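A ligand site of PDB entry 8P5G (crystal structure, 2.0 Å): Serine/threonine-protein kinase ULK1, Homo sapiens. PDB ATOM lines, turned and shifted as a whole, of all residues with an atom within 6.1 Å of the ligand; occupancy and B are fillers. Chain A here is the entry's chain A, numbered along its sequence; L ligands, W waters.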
ATOM      1  N   ILE A  23      37.352 -29.830  -9.343  1.00  0.00           N
ATOM      2  CA  ILE A  23      36.603 -28.819 -10.063  1.00  0.00           C
ATOM      3  C   ILE A  23      36.357 -27.659  -9.132  1.00  0.00           C
ATOM      4  O   ILE A  23      36.512 -26.509  -9.511  1.00  0.00           O
ATOM      5  CB  ILE A  23      35.268 -29.359 -10.597  1.00  0.00           C
ATOM      6  CG1 ILE A  23      35.489 -30.355 -11.729  1.00  0.00           C
ATOM      7  CG2 ILE A  23      34.352 -28.221 -11.005  1.00  0.00           C
ATOM      8  CD1 ILE A  23      34.234 -31.072 -12.191  1.00  0.00           C
ATOM      9  N   GLY A  24      35.967 -27.959  -7.897  1.00  0.00           N
ATOM     10  CA  GLY A  24      35.915 -26.956  -6.852  1.00  0.00           C
ATOM     11  C   GLY A  24      35.209 -27.484  -5.613  1.00  0.00           C
ATOM     12  O   GLY A  24      34.824 -28.651  -5.552  1.00  0.00           O
ATOM     13  N   HIS A  25      35.069 -26.612  -4.628  1.00  0.00           N
ATOM     14  CA  HIS A  25      34.448 -26.981  -3.376  1.00  0.00           C
ATOM     15  C   HIS A  25      33.612 -25.809  -2.909  1.00  0.00           C
ATOM     16  O   HIS A  25      33.887 -24.684  -3.267  1.00  0.00           O
ATOM     17  CB  HIS A  25      35.495 -27.377  -2.318  1.00  0.00           C
ATOM     18  CG  HIS A  25      36.331 -26.242  -1.828  1.00  0.00           C
ATOM     19  ND1 HIS A  25      37.486 -25.870  -2.487  1.00  0.00           N
ATOM     20  CD2 HIS A  25      36.197 -25.436  -0.763  1.00  0.00           C
ATOM     21  CE1 HIS A  25      38.022 -24.831  -1.835  1.00  0.00           C
ATOM     22  NE2 HIS A  25      37.259 -24.559  -0.790  1.00  0.00           N
ATOM     23  N   GLY A  26      32.568 -26.119  -2.158  1.00  0.00           N
ATOM     24  CA  GLY A  26      31.890 -25.170  -1.299  1.00  0.00           C
ATOM     25  C   GLY A  26      31.758 -25.826   0.070  1.00  0.00           C
ATOM     26  O   GLY A  26      32.278 -26.924   0.280  1.00  0.00           O
ATOM     27  N   ALA A  29      29.966 -29.437  -0.327  1.00  0.00           N
ATOM     28  CA  ALA A  29      30.300 -30.408  -1.354  1.00  0.00           C
ATOM     29  C   ALA A  29      31.675 -30.103  -1.939  1.00  0.00           C
ATOM     30  O   ALA A  29      32.099 -28.946  -1.969  1.00  0.00           O
ATOM     31  CB  ALA A  29      29.252 -30.366  -2.420  1.00  0.00           C
ATOM     32  N   VAL A  31      33.667 -31.161  -5.620  1.00  0.00           N
ATOM     33  CA  VAL A  31      33.362 -31.737  -6.929  1.00  0.00           C
ATOM     34  C   VAL A  31      34.665 -32.040  -7.650  1.00  0.00           C
ATOM     35  O   VAL A  31      35.531 -31.179  -7.700  1.00  0.00           O
ATOM     36  CB  VAL A  31      32.485 -30.790  -7.748  1.00  0.00           C
ATOM     37  CG1 VAL A  31      32.046 -31.412  -9.058  1.00  0.00           C
ATOM     38  CG2 VAL A  31      31.288 -30.300  -6.951  1.00  0.00           C
ATOM     39  N   ALA A  45      31.025 -35.184 -13.597  1.00  0.00           N
ATOM     40  CA  ALA A  45      31.424 -34.545 -12.369  1.00  0.00           C
ATOM     41  C   ALA A  45      30.969 -35.429 -11.204  1.00  0.00           C
ATOM     42  O   ALA A  45      29.842 -35.939 -11.215  1.00  0.00           O
ATOM     43  CB  ALA A  45      30.764 -33.207 -12.303  1.00  0.00           C
ATOM     44  N   LYS A  47      30.341 -35.443  -7.232  1.00  0.00           N
ATOM     45  CA  LYS A  47      30.160 -34.614  -6.058  1.00  0.00           C
ATOM     46  C   LYS A  47      30.266 -35.492  -4.816  1.00  0.00           C
ATOM     47  O   LYS A  47      29.675 -36.571  -4.776  1.00  0.00           O
ATOM     48  CB  LYS A  47      28.810 -33.913  -6.249  1.00  0.00           C
ATOM     49  CG  LYS A  47      28.441 -32.797  -5.290  1.00  0.00           C
ATOM     50  CD  LYS A  47      27.268 -31.969  -5.828  1.00  0.00           C
ATOM     51  CE  LYS A  47      26.783 -30.949  -4.810  1.00  0.00           C
ATOM     52  NZ  LYS A  47      25.523 -30.282  -5.216  1.00  0.00           N
ATOM     53  N   GLU A  64      19.857 -34.327  -2.098  1.00  0.00           N
ATOM     54  CA  GLU A  64      19.976 -34.027  -3.514  1.00  0.00           C
ATOM     55  C   GLU A  64      19.735 -35.277  -4.345  1.00  0.00           C
ATOM     56  O   GLU A  64      19.060 -35.238  -5.378  1.00  0.00           O
ATOM     57  CB  GLU A  64      21.319 -33.378  -3.815  1.00  0.00           C
ATOM     58  CG  GLU A  64      21.453 -33.037  -5.278  1.00  0.00           C
ATOM     59  CD  GLU A  64      22.609 -32.111  -5.587  1.00  0.00           C
ATOM     60  OE1 GLU A  64      23.611 -32.115  -4.796  1.00  0.00           O
ATOM     61  OE2 GLU A  64      22.510 -31.388  -6.621  1.00  0.00           O
ATOM     62  N   VAL A  77      20.626 -30.784 -14.483  1.00  0.00           N
ATOM     63  CA  VAL A  77      21.840 -31.585 -14.553  1.00  0.00           C
ATOM     64  C   VAL A  77      21.480 -33.041 -14.252  1.00  0.00           C
ATOM     65  O   VAL A  77      20.770 -33.329 -13.299  1.00  0.00           O
ATOM     66  CB  VAL A  77      22.940 -31.061 -13.616  1.00  0.00           C
ATOM     67  CG1 VAL A  77      24.258 -31.756 -13.907  1.00  0.00           C
ATOM     68  CG2 VAL A  77      23.147 -29.564 -13.698  1.00  0.00           C
ATOM     69  N   MET A  93      27.328 -37.001 -11.949  1.00  0.00           N
ATOM     70  CA  MET A  93      26.544 -36.158 -12.830  1.00  0.00           C
ATOM     71  C   MET A  93      27.217 -35.895 -14.166  1.00  0.00           C
ATOM     72  O   MET A  93      28.439 -35.972 -14.293  1.00  0.00           O
ATOM     73  CB  MET A  93      26.293 -34.843 -12.107  1.00  0.00           C
ATOM     74  CG  MET A  93      25.247 -35.075 -10.997  1.00  0.00           C
ATOM     75  SD  MET A  93      25.135 -33.693  -9.916  1.00  0.00           S
ATOM     76  CE  MET A  93      26.817 -33.554  -9.339  1.00  0.00           C
ATOM     77  N   GLU A  94      26.371 -35.600 -15.163  1.00  0.00           N
ATOM     78  CA  GLU A  94      26.832 -35.107 -16.449  1.00  0.00           C
ATOM     79  C   GLU A  94      27.763 -33.929 -16.190  1.00  0.00           C
ATOM     80  O   GLU A  94      27.500 -33.099 -15.321  1.00  0.00           O
ATOM     81  CB  GLU A  94      25.666 -34.778 -17.390  1.00  0.00           C
ATOM     82  CG  GLU A  94      24.990 -33.436 -17.163  1.00  0.00           C
ATOM     83  CD  GLU A  94      23.808 -33.178 -18.094  1.00  0.00           C
ATOM     84  OE1 GLU A  94      22.678 -32.890 -17.602  1.00  0.00           O
ATOM     85  OE2 GLU A  94      23.990 -33.269 -19.330  1.00  0.00           O
ATOM     86  N   TYR A  95      28.884 -33.924 -16.914  1.00  0.00           N
ATOM     87  CA  TYR A  95      29.858 -32.860 -16.832  1.00  0.00           C
ATOM     88  C   TYR A  95      29.351 -31.657 -17.630  1.00  0.00           C
ATOM     89  O   TYR A  95      28.964 -31.834 -18.748  1.00  0.00           O
ATOM     90  CB  TYR A  95      31.205 -33.285 -17.420  1.00  0.00           C
ATOM     91  CG  TYR A  95      32.294 -32.247 -17.296  1.00  0.00           C
ATOM     92  CD1 TYR A  95      32.675 -31.812 -16.053  1.00  0.00           C
ATOM     93  CD2 TYR A  95      32.922 -31.706 -18.401  1.00  0.00           C
ATOM     94  CE1 TYR A  95      33.713 -30.898 -15.880  1.00  0.00           C
ATOM     95  CE2 TYR A  95      33.934 -30.755 -18.256  1.00  0.00           C
ATOM     96  CZ  TYR A  95      34.333 -30.363 -17.004  1.00  0.00           C
ATOM     97  OH  TYR A  95      35.308 -29.429 -16.730  1.00  0.00           O
ATOM     98  N   CYS A  96      29.350 -30.467 -17.060  1.00  0.00           N
ATOM     99  CA  CYS A  96      28.847 -29.297 -17.760  1.00  0.00           C
ATOM    100  C   CYS A  96      30.056 -28.451 -18.191  1.00  0.00           C
ATOM    101  O   CYS A  96      30.633 -27.756 -17.387  1.00  0.00           O
ATOM    102  CB  CYS A  96      27.886 -28.516 -16.874  1.00  0.00           C
ATOM    103  SG  CYS A  96      26.346 -29.456 -16.608  1.00  0.00           S
ATOM    104  N   ASN A  97      30.424 -28.538 -19.457  1.00  0.00           N
ATOM    105  CA  ASN A  97      31.753 -28.071 -19.874  1.00  0.00           C
ATOM    106  C   ASN A  97      31.820 -26.548 -20.004  1.00  0.00           C
ATOM    107  O   ASN A  97      32.896 -26.044 -20.264  1.00  0.00           O
ATOM    108  CB  ASN A  97      32.197 -28.736 -21.167  1.00  0.00           C
ATOM    109  CG  ASN A  97      31.266 -28.453 -22.314  1.00  0.00           C
ATOM    110  OD1 ASN A  97      30.356 -27.635 -22.203  1.00  0.00           O
ATOM    111  ND2 ASN A  97      31.490 -29.097 -23.430  1.00  0.00           N
ATOM    112  N   GLY A  98      30.750 -25.807 -19.674  1.00  0.00           N
ATOM    113  CA  GLY A  98      30.744 -24.344 -19.737  1.00  0.00           C
ATOM    114  C   GLY A  98      30.951 -23.660 -18.385  1.00  0.00           C
ATOM    115  O   GLY A  98      30.995 -22.434 -18.308  1.00  0.00           O
ATOM    116  N   GLY A  99      31.009 -24.434 -17.300  1.00  0.00           N
ATOM    117  CA  GLY A  99      31.060 -23.851 -15.976  1.00  0.00           C
ATOM    118  C   GLY A  99      29.688 -23.299 -15.545  1.00  0.00           C
ATOM    119  O   GLY A  99      28.663 -23.743 -16.055  1.00  0.00           O
ATOM    120  N   ASP A 100      29.672 -22.297 -14.675  1.00  0.00           N
ATOM    121  CA  ASP A 100      28.380 -21.798 -14.200  1.00  0.00           C
ATOM    122  C   ASP A 100      28.095 -20.385 -14.691  1.00  0.00           C
ATOM    123  O   ASP A 100      28.985 -19.670 -15.193  1.00  0.00           O
ATOM    124  CB  ASP A 100      28.319 -21.914 -12.677  1.00  0.00           C
ATOM    125  CG  ASP A 100      29.246 -20.979 -11.933  1.00  0.00           C
ATOM    126  OD1 ASP A 100      29.568 -19.925 -12.482  1.00  0.00           O
ATOM    127  OD2 ASP A 100      29.668 -21.340 -10.814  1.00  0.00           O
ATOM    128  N   ASP A 103      30.173 -17.320 -13.349  1.00  0.00           N
ATOM    129  CA  ASP A 103      31.466 -17.008 -13.956  1.00  0.00           C
ATOM    130  C   ASP A 103      31.258 -16.389 -15.342  1.00  0.00           C
ATOM    131  O   ASP A 103      31.934 -15.422 -15.684  1.00  0.00           O
ATOM    132  CB  ASP A 103      32.334 -18.251 -14.070  1.00  0.00           C
ATOM    133  CG  ASP A 103      32.927 -18.701 -12.746  1.00  0.00           C
ATOM    134  OD1 ASP A 103      32.862 -17.930 -11.776  1.00  0.00           O
ATOM    135  OD2 ASP A 103      33.449 -19.794 -12.722  1.00  0.00           O
ATOM    136  N   PRO A 142      22.930 -17.782  -9.958  1.00  0.00           N
ATOM    137  CA  PRO A 142      23.793 -18.092 -11.105  1.00  0.00           C
ATOM    138  C   PRO A 142      24.843 -19.157 -10.847  1.00  0.00           C
ATOM    139  O   PRO A 142      25.227 -19.884 -11.764  1.00  0.00           O
ATOM    140  CB  PRO A 142      24.458 -16.721 -11.437  1.00  0.00           C
ATOM    141  CG  PRO A 142      23.390 -15.743 -10.926  1.00  0.00           C
ATOM    142  CD  PRO A 142      22.951 -16.359  -9.617  1.00  0.00           C
ATOM    143  N   GLN A 143      25.289 -19.276  -9.592  1.00  0.00           N
ATOM    144  CA  GLN A 143      26.271 -20.277  -9.203  1.00  0.00           C
ATOM    145  C   GLN A 143      25.692 -21.688  -9.345  1.00  0.00           C
ATOM    146  O   GLN A 143      26.481 -22.628  -9.454  1.00  0.00           O
ATOM    147  CB  GLN A 143      26.740 -20.092  -7.757  1.00  0.00           C
ATOM    148  CG  GLN A 143      27.538 -18.802  -7.540  1.00  0.00           C
ATOM    149  CD  GLN A 143      26.710 -17.540  -7.359  1.00  0.00           C
ATOM    150  OE1 GLN A 143      25.489 -17.478  -7.538  1.00  0.00           O
ATOM    151  NE2 GLN A 143      27.422 -16.476  -7.022  1.00  0.00           N
ATOM    152  N   ASN A 144      24.365 -21.821  -9.405  1.00  0.00           N
ATOM    153  CA  ASN A 144      23.716 -23.132  -9.439  1.00  0.00           C
ATOM    154  C   ASN A 144      23.072 -23.365 -10.794  1.00  0.00           C
ATOM    155  O   ASN A 144      22.224 -24.261 -10.932  1.00  0.00           O
ATOM    156  CB  ASN A 144      22.676 -23.257  -8.318  1.00  0.00           C
ATOM    157  CG  ASN A 144      23.330 -23.384  -6.965  1.00  0.00           C
ATOM    158  OD1 ASN A 144      24.496 -23.697  -6.896  1.00  0.00           O
ATOM    159  ND2 ASN A 144      22.585 -23.132  -5.907  1.00  0.00           N
ATOM    160  N   LEU A 146      24.296 -24.149 -14.596  1.00  0.00           N
ATOM    161  CA  LEU A 146      25.491 -24.580 -15.297  1.00  0.00           C
ATOM    162  C   LEU A 146      25.253 -24.458 -16.806  1.00  0.00           C
ATOM    163  O   LEU A 146      24.134 -24.507 -17.269  1.00  0.00           O
ATOM    164  CB  LEU A 146      25.811 -26.031 -14.936  1.00  0.00           C
ATOM    165  CG  LEU A 146      25.999 -26.372 -13.460  1.00  0.00           C
ATOM    166  CD1 LEU A 146      26.282 -27.845 -13.261  1.00  0.00           C
ATOM    167  CD2 LEU A 146      27.101 -25.575 -12.834  1.00  0.00           C
ATOM    168  N   ALA A 165      21.219 -26.885 -11.264  1.00  0.00           N
ATOM    169  CA  ALA A 165      21.986 -27.782 -10.431  1.00  0.00           C
ATOM    170  C   ALA A 165      21.757 -27.447  -8.959  1.00  0.00           C
ATOM    171  O   ALA A 165      21.029 -26.502  -8.623  1.00  0.00           O
ATOM    172  CB  ALA A 165      23.459 -27.692 -10.757  1.00  0.00           C
ATOM    173  N   ASP A 166      22.340 -28.314  -8.101  1.00  0.00           N
ATOM    174  CA  ASP A 166      22.448 -28.070  -6.658  1.00  0.00           C
ATOM    175  C   ASP A 166      21.054 -28.092  -6.024  1.00  0.00           C
ATOM    176  O   ASP A 166      20.568 -27.087  -5.541  1.00  0.00           O
ATOM    177  CB  ASP A 166      23.302 -26.824  -6.379  1.00  0.00           C
ATOM    178  CG  ASP A 166      24.811 -27.128  -6.353  1.00  0.00           C
ATOM    179  OD1 ASP A 166      25.286 -28.043  -7.149  1.00  0.00           O
ATOM    180  OD2 ASP A 166      25.514 -26.507  -5.518  1.00  0.00           O
HETATM  181  C1  LIG L   1      33.202 -24.979 -12.883  1.00  0.00           C
HETATM  182  C2  LIG L   1      33.899 -24.875 -14.058  1.00  0.00           C
HETATM  183  C3  LIG L   1      33.680 -25.841 -15.078  1.00  0.00           C
HETATM  184  C4  LIG L   1      32.792 -26.871 -14.890  1.00  0.00           C
HETATM  185  C5  LIG L   1      32.045 -26.976 -13.694  1.00  0.00           C
HETATM  186  N1  LIG L   1      31.147 -28.009 -13.535  1.00  0.00           N
HETATM  187  C6  LIG L   1      30.491 -28.074 -12.393  1.00  0.00           C
HETATM  188  N2  LIG L   1      30.569 -27.150 -11.403  1.00  0.00           N
HETATM  189  C7  LIG L   1      31.452 -26.171 -11.496  1.00  0.00           C
HETATM  190  C8  LIG L   1      32.248 -26.013 -12.682  1.00  0.00           C
HETATM  191  N3  LIG L   1      31.506 -25.303 -10.501  1.00  0.00           N
HETATM  192  C9  LIG L   1      30.559 -25.368  -9.421  1.00  0.00           C
HETATM  193  C10 LIG L   1      30.983 -24.413  -8.271  1.00  0.00           C
HETATM  194  C11 LIG L   1      29.777 -23.511  -8.026  1.00  0.00           C
HETATM  195  N4  LIG L   1      28.999 -23.557  -9.272  1.00  0.00           N
HETATM  196  C12 LIG L   1      29.128 -24.936  -9.783  1.00  0.00           C
HETATM  197  C13 LIG L   1      31.359 -25.293  -7.068  1.00  0.00           C
HETATM  198  C14 LIG L   1      32.510 -26.217  -7.389  1.00  0.00           C
HETATM  199  C15 LIG L   1      31.656 -24.463  -5.821  1.00  0.00           C
HETATM  200  O1  LIG L   1      30.226 -26.141  -6.759  1.00  0.00           O
HETATM  201  C16 LIG L   1      29.477 -29.125 -12.181  1.00  0.00           C
HETATM  202  C17 LIG L   1      29.146 -30.003 -13.211  1.00  0.00           C
HETATM  203  C18 LIG L   1      28.153 -30.957 -13.068  1.00  0.00           C
HETATM  204  C19 LIG L   1      27.474 -31.060 -11.876  1.00  0.00           C
HETATM  205  C20 LIG L   1      27.820 -30.222 -10.847  1.00  0.00           C
HETATM  206  C21 LIG L   1      28.813 -29.259 -10.968  1.00  0.00           C
HETATM  207  F1  LIG L   1      27.145 -30.325  -9.677  1.00  0.00           F
HETATM  208  O2  LIG L   1      29.838 -29.899 -14.364  1.00  0.00           O
HETATM  209  O3  LIG L   1      34.425 -25.599 -16.184  1.00  0.00           O
HETATM  210  C22 LIG L   1      34.132 -26.371 -17.357  1.00  0.00           C
HETATM  211  O4  LIG L   1      34.813 -23.922 -14.382  1.00  0.00           O
HETATM  212  C23 LIG L   1      35.235 -23.056 -13.333  1.00  0.00           C
HETATM  213  O   HOH W   1      23.836 -30.843  -8.680  1.00  0.00           O
HETATM  214  O   HOH W   2      32.704 -22.356 -10.669  1.00  0.00           O
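O of Gln 143 sits at hydrogen-bond distance from N4 of the ligand (2.7 Å). A nitrogen (N4) of the ligand lies within salt-bridge range of the side-chain carboxylate of Asp 100 (2.8 Å). N of Cys 96 lies within hydrogen-bond range of O2 of the ligand, 2.8 Å away.
N of Asp 103 sits at hydrogen-bond distance from OD1 of Asp 100 (2.8 Å). The backbone NH of Ala 45 lies within hydrogen-bond range of the backbone carbonyl oxygen of Met 93 (2.8 Å). The backbone carbonyl oxygen of Gly 24 sits at hydrogen-bond distance from the backbone NH of Val 31, 2.8 Å away. The backbone NH (N) of Ile 23 sits at hydrogen-bond distance from the backbone carbonyl oxygen (O) of Val 31 (2.8 Å). OD1 of Asp 166 is in salt-bridge range of NZ of Lys 47, at 3.0 Å. The side-chain carboxylate (OD2) of Asp 166 sits close to the side-chain amide oxygen (OD1) of Asn 144. OE2 of Glu 64 sits close to N of Asp 166, at 3.4 Å.
CG2 of Ile 23 touches C8 of the ligand (3.5 Å). C of Gly 24 touches C14 of the ligand, at 3.5 Å. His 25 touches the ligand. Ala 45 touches the ligand. Val 77 touches the ligand. Met 93 touches the ligand (CE to F1, 3.3 Å). Glu 94 touches the ligand (O to C18, 3.2 Å). Tyr 95 touches the ligand (OH to C22, 3.3 Å). O of Asn 97 touches C22 of the ligand, at 3.2 Å. Gly 99 touches the ligand (CA to C3, 3.4 Å). Asp 103 touches the ligand. Leu 146 touches the ligand (CD1 to C17, 3.6 Å). Asp 166 touches the ligand. Of the 25 residues printed, 16 come within 4 Å of the ligand. The nearest printed residue that does not touch the ligand is Gly 26 (4.1 Å).
Water W2 lies within hydrogen-bond range of a nitrogen (N3) of the ligand (3.2 Å), the side-chain carboxylate of Asp 100 (3.2 Å) and the side-chain carboxylate of Asp 103 (3.4 Å). Water W1 lies within hydrogen-bond range of OE2 of Glu 64, N of Asp 166 and SD of Met 93.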
